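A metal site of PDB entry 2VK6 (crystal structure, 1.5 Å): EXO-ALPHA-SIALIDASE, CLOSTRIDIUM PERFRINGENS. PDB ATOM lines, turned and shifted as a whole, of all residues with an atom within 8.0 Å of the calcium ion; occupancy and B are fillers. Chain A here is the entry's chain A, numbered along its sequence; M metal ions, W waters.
The backbone NH (N) of Arg 44 is in hydrogen-bond range of the backbone carbonyl oxygen (O) of Asp 54 (3.0 Å). The side-chain carboxylate (OD2) of Asp 54 sits at hydrogen-bond distance from the backbone NH (N) of Lys 81. The side-chain carboxylate (OD2) of Asp 56 lies within salt-bridge range of the guanidinium group (NH1) of Arg 44, at 2.9 Å. O of Asp 56 is in hydrogen-bond range of N of Ala 42, 2.8 Å away.
Four residues have an atom within 4 Å of the calcium ion: Asp 54, Asp 56, Asp 77 and Tyr 78. The nearest printed residue that does not touch the calcium ion is Ser 82 (4.3 Å).
The calcium ion is bound by the side-chain carboxylate of Asp 54, the backbone carbonyl oxygen of Tyr 78, the side-chain carboxylate of Asp 77, the side-chain carboxylate of Asp 56, water W3, water W1 and water W2. The calcium ion has seven donor atoms within binding distance.
Water W2 lies within hydrogen-bond range of O of Ser 82, O of Ile 55 and N of Tyr 78.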
ATOM      1  N   ALA A  42      -8.460  16.682  15.339  1.00  0.00           N
ATOM      2  CA  ALA A  42      -9.207  16.817  14.107  1.00  0.00           C
ATOM      3  C   ALA A  42     -10.698  16.741  14.486  1.00  0.00           C
ATOM      4  O   ALA A  42     -11.250  15.651  14.718  1.00  0.00           O
ATOM      5  CB  ALA A  42      -8.832  15.635  13.173  1.00  0.00           C
ATOM      6  N   ARG A  44     -14.374  16.823  13.620  1.00  0.00           N
ATOM      7  CA  ARG A  44     -14.924  16.508  12.302  1.00  0.00           C
ATOM      8  C   ARG A  44     -16.279  17.131  12.044  1.00  0.00           C
ATOM      9  O   ARG A  44     -16.708  17.208  10.871  1.00  0.00           O
ATOM     10  CB  ARG A  44     -14.983  14.991  12.048  1.00  0.00           C
ATOM     11  CG  ARG A  44     -13.699  14.214  12.363  1.00  0.00           C
ATOM     12  CD  ARG A  44     -12.533  14.650  11.486  1.00  0.00           C
ATOM     13  NE  ARG A  44     -12.752  14.428  10.053  1.00  0.00           N
ATOM     14  CZ  ARG A  44     -12.458  13.288   9.446  1.00  0.00           C
ATOM     15  NH1 ARG A  44     -11.942  12.284  10.155  1.00  0.00           N
ATOM     16  NH2 ARG A  44     -12.665  13.144   8.150  1.00  0.00           N
ATOM     17  N   HIS A  45     -16.969  17.570  13.095  1.00  0.00           N
ATOM     18  CA  HIS A  45     -18.322  18.128  12.933  1.00  0.00           C
ATOM     19  C   HIS A  45     -18.433  19.468  13.560  1.00  0.00           C
ATOM     20  O   HIS A  45     -19.280  19.687  14.410  1.00  0.00           O
ATOM     21  CB  HIS A  45     -19.396  17.195  13.530  1.00  0.00           C
ATOM     22  CG  HIS A  45     -19.396  15.830  12.952  1.00  0.00           C
ATOM     23  ND1 HIS A  45     -19.478  15.581  11.594  1.00  0.00           N
ATOM     24  CD2 HIS A  45     -19.338  14.612  13.548  1.00  0.00           C
ATOM     25  CE1 HIS A  45     -19.416  14.272  11.383  1.00  0.00           C
ATOM     26  NE2 HIS A  45     -19.335  13.670  12.553  1.00  0.00           N
ATOM     27  N   ASN A  53     -19.568  16.378  19.127  1.00  0.00           N
ATOM     28  CA  ASN A  53     -18.636  16.276  18.016  1.00  0.00           C
ATOM     29  C   ASN A  53     -18.208  14.828  17.814  1.00  0.00           C
ATOM     30  O   ASN A  53     -18.605  13.936  18.562  1.00  0.00           O
ATOM     31  CB  ASN A  53     -17.389  17.169  18.270  1.00  0.00           C
ATOM     32  CG  ASN A  53     -16.890  17.838  17.006  1.00  0.00           C
ATOM     33  OD1 ASN A  53     -16.947  17.246  15.911  1.00  0.00           O
ATOM     34  ND2 ASN A  53     -16.349  19.016  17.146  1.00  0.00           N
ATOM     35  N   ASP A  54     -17.360  14.654  16.806  1.00  0.00           N
ATOM     36  CA  ASP A  54     -16.627  13.380  16.601  1.00  0.00           C
ATOM     37  C   ASP A  54     -15.196  13.815  16.327  1.00  0.00           C
ATOM     38  O   ASP A  54     -14.913  14.420  15.274  1.00  0.00           O
ATOM     39  CB  ASP A  54     -17.203  12.617  15.387  1.00  0.00           C
ATOM     40  CG  ASP A  54     -16.737  11.155  15.352  1.00  0.00           C
ATOM     41  OD1 ASP A  54     -15.533  10.965  15.608  1.00  0.00           O
ATOM     42  OD2 ASP A  54     -17.538  10.222  15.039  1.00  0.00           O
ATOM     43  N   ILE A  55     -14.334  13.568  17.301  1.00  0.00           N
ATOM     44  CA  ILE A  55     -12.981  14.137  17.272  1.00  0.00           C
ATOM     45  C   ILE A  55     -11.963  12.994  17.252  1.00  0.00           C
ATOM     46  O   ILE A  55     -12.065  11.984  18.006  1.00  0.00           O
ATOM     47  CB  ILE A  55     -12.710  15.061  18.526  1.00  0.00           C
ATOM     48  CG1 ILE A  55     -13.824  16.110  18.696  1.00  0.00           C
ATOM     49  CG2 ILE A  55     -11.328  15.738  18.384  1.00  0.00           C
ATOM     50  CD1 ILE A  55     -13.736  16.868  20.051  1.00  0.00           C
ATOM     51  N   ASP A  56     -11.031  13.150  16.307  1.00  0.00           N
ATOM     52  CA  ASP A  56      -9.911  12.198  16.090  1.00  0.00           C
ATOM     53  C   ASP A  56      -8.596  12.925  16.385  1.00  0.00           C
ATOM     54  O   ASP A  56      -8.573  14.154  16.420  1.00  0.00           O
ATOM     55  CB  ASP A  56      -9.881  11.785  14.609  1.00  0.00           C
ATOM     56  CG  ASP A  56     -11.198  11.175  14.128  1.00  0.00           C
ATOM     57  OD1 ASP A  56     -11.894  10.535  14.941  1.00  0.00           O
ATOM     58  OD2 ASP A  56     -11.523  11.372  12.925  1.00  0.00           O
ATOM     59  N   THR A  57      -7.525  12.172  16.595  1.00  0.00           N
ATOM     60  CA  THR A  57      -6.217  12.811  16.851  1.00  0.00           C
ATOM     61  C   THR A  57      -5.389  12.736  15.568  1.00  0.00           C
ATOM     62  O   THR A  57      -5.229  11.636  14.989  1.00  0.00           O
ATOM     63  CB  THR A  57      -5.432  12.041  17.948  1.00  0.00           C
ATOM     64  OG1 THR A  57      -6.159  12.084  19.172  1.00  0.00           O
ATOM     65  CG2 THR A  57      -4.094  12.711  18.178  1.00  0.00           C
ATOM     66  N   ILE A  74      -3.929  10.321  10.876  1.00  0.00           N
ATOM     67  CA  ILE A  74      -4.841  10.173  11.994  1.00  0.00           C
ATOM     68  C   ILE A  74      -4.380   8.982  12.787  1.00  0.00           C
ATOM     69  O   ILE A  74      -4.217   7.865  12.228  1.00  0.00           O
ATOM     70  CB  ILE A  74      -6.330   9.965  11.515  1.00  0.00           C
ATOM     71  CG1 ILE A  74      -6.823  11.133  10.662  1.00  0.00           C
ATOM     72  CG2 ILE A  74      -7.235   9.568  12.692  1.00  0.00           C
ATOM     73  CD1 ILE A  74      -6.975  12.436  11.395  1.00  0.00           C
ATOM     74  N   MET A  76      -5.672   8.181  16.182  1.00  0.00           N
ATOM     75  CA  MET A  76      -6.725   7.577  16.994  1.00  0.00           C
ATOM     76  C   MET A  76      -8.058   8.092  16.473  1.00  0.00           C
ATOM     77  O   MET A  76      -8.190   9.264  16.208  1.00  0.00           O
ATOM     78  CB  MET A  76      -6.622   7.982  18.474  1.00  0.00           C
ATOM     79  CG  MET A  76      -5.627   7.079  19.242  1.00  0.00           C
ATOM     80  SD  MET A  76      -5.418   7.595  20.972  1.00  0.00           S
ATOM     81  CE  MET A  76      -4.354   8.994  20.627  1.00  0.00           C
ATOM     82  N   ASP A  77      -9.016   7.162  16.307  1.00  0.00           N
ATOM     83  CA  ASP A  77     -10.317   7.442  15.679  1.00  0.00           C
ATOM     84  C   ASP A  77     -11.290   6.396  16.266  1.00  0.00           C
ATOM     85  O   ASP A  77     -11.100   5.174  16.073  1.00  0.00           O
ATOM     86  CB  ASP A  77     -10.200   7.344  14.128  1.00  0.00           C
ATOM     87  CG  ASP A  77     -11.546   7.485  13.391  1.00  0.00           C
ATOM     88  OD1 ASP A  77     -12.632   7.601  13.992  1.00  0.00           O
ATOM     89  OD2 ASP A  77     -11.519   7.442  12.142  1.00  0.00           O
ATOM     90  N   TYR A  78     -12.276   6.883  17.023  1.00  0.00           N
ATOM     91  CA  TYR A  78     -13.333   5.993  17.518  1.00  0.00           C
ATOM     92  C   TYR A  78     -14.622   6.337  16.743  1.00  0.00           C
ATOM     93  O   TYR A  78     -14.778   7.437  16.184  1.00  0.00           O
ATOM     94  CB  TYR A  78     -13.565   6.259  19.026  1.00  0.00           C
ATOM     95  CG  TYR A  78     -12.430   5.795  19.873  1.00  0.00           C
ATOM     96  CD1 TYR A  78     -11.323   6.627  20.122  1.00  0.00           C
ATOM     97  CD2 TYR A  78     -12.437   4.517  20.399  1.00  0.00           C
ATOM     98  CE1 TYR A  78     -10.230   6.155  20.870  1.00  0.00           C
ATOM     99  CE2 TYR A  78     -11.357   4.057  21.208  1.00  0.00           C
ATOM    100  CZ  TYR A  78     -10.286   4.910  21.464  1.00  0.00           C
ATOM    101  OH  TYR A  78      -9.246   4.480  22.240  1.00  0.00           O
ATOM    102  N   PRO A  79     -15.550   5.372  16.689  1.00  0.00           N
ATOM    103  CA  PRO A  79     -16.760   5.586  15.902  1.00  0.00           C
ATOM    104  C   PRO A  79     -17.882   6.345  16.617  1.00  0.00           C
ATOM    105  O   PRO A  79     -17.876   6.474  17.844  1.00  0.00           O
ATOM    106  CB  PRO A  79     -17.250   4.140  15.639  1.00  0.00           C
ATOM    107  CG  PRO A  79     -16.842   3.375  16.890  1.00  0.00           C
ATOM    108  CD  PRO A  79     -15.479   4.013  17.307  1.00  0.00           C
ATOM    109  N   ASP A  80     -18.858   6.834  15.818  1.00  0.00           N
ATOM    110  CA  ASP A  80     -20.186   7.219  16.357  1.00  0.00           C
ATOM    111  C   ASP A  80     -20.095   8.254  17.441  1.00  0.00           C
ATOM    112  O   ASP A  80     -20.863   8.196  18.425  1.00  0.00           O
ATOM    113  CB  ASP A  80     -20.954   5.994  16.860  1.00  0.00           C
ATOM    114  CG  ASP A  80     -22.448   6.252  17.029  1.00  0.00           C
ATOM    115  OD1 ASP A  80     -22.993   7.175  16.380  1.00  0.00           O
ATOM    116  OD2 ASP A  80     -23.034   5.507  17.875  1.00  0.00           O
ATOM    117  N   LYS A  81     -19.272   9.280  17.198  1.00  0.00           N
ATOM    118  CA  LYS A  81     -19.207  10.451  18.093  1.00  0.00           C
ATOM    119  C   LYS A  81     -18.540  10.134  19.457  1.00  0.00           C
ATOM    120  O   LYS A  81     -18.697  10.885  20.444  1.00  0.00           O
ATOM    121  CB  LYS A  81     -20.569  11.153  18.249  1.00  0.00           C
ATOM    122  CG  LYS A  81     -21.033  11.714  16.899  1.00  0.00           C
ATOM    123  CD  LYS A  81     -22.315  12.568  17.033  1.00  0.00           C
ATOM    124  CE  LYS A  81     -22.030  13.990  17.536  1.00  0.00           C
ATOM    125  NZ  LYS A  81     -23.324  14.707  17.891  1.00  0.00           N
ATOM    126  N   SER A  82     -17.855   8.977  19.547  1.00  0.00           N
ATOM    127  CA  SER A  82     -16.874   8.811  20.633  1.00  0.00           C
ATOM    128  C   SER A  82     -15.626   9.605  20.238  1.00  0.00           C
ATOM    129  O   SER A  82     -15.187   9.508  19.075  1.00  0.00           O
ATOM    130  CB  SER A  82     -16.501   7.337  20.793  1.00  0.00           C
ATOM    131  OG  SER A  82     -15.485   7.193  21.758  1.00  0.00           O
ATOM    132  N   SER A  83     -15.116  10.438  21.147  1.00  0.00           N
ATOM    133  CA  SER A  83     -14.053  11.390  20.786  1.00  0.00           C
ATOM    134  C   SER A  83     -12.780  11.152  21.613  1.00  0.00           C
ATOM    135  O   SER A  83     -12.884  10.808  22.830  1.00  0.00           O
ATOM    136  CB  SER A  83     -14.483  12.833  21.089  1.00  0.00           C
ATOM    137  OG  SER A  83     -15.370  13.262  20.058  1.00  0.00           O
ATOM    138  N   VAL A  84     -11.643  11.481  20.986  1.00  0.00           N
ATOM    139  CA  VAL A  84     -10.375  11.707  21.701  1.00  0.00           C
ATOM    140  C   VAL A  84     -10.122  13.213  21.615  1.00  0.00           C
ATOM    141  O   VAL A  84     -10.231  13.809  20.526  1.00  0.00           O
ATOM    142  CB  VAL A  84      -9.170  10.903  21.113  1.00  0.00           C
ATOM    143  CG1 VAL A  84      -9.136   9.472  21.641  1.00  0.00           C
ATOM    144  CG2 VAL A  84      -9.217  10.870  19.606  1.00  0.00           C
HETATM  145 CA    CA M   1     -14.004   9.304  14.959  1.00  0.00          CA
HETATM  146  O   HOH W   1     -15.986   8.480  13.699  1.00  0.00           O
HETATM  147  O   HOH W   2     -13.163   9.621  17.327  1.00  0.00           O
HETATM  148  O   HOH W   3     -13.965  10.364  12.730  1.00  0.00           O
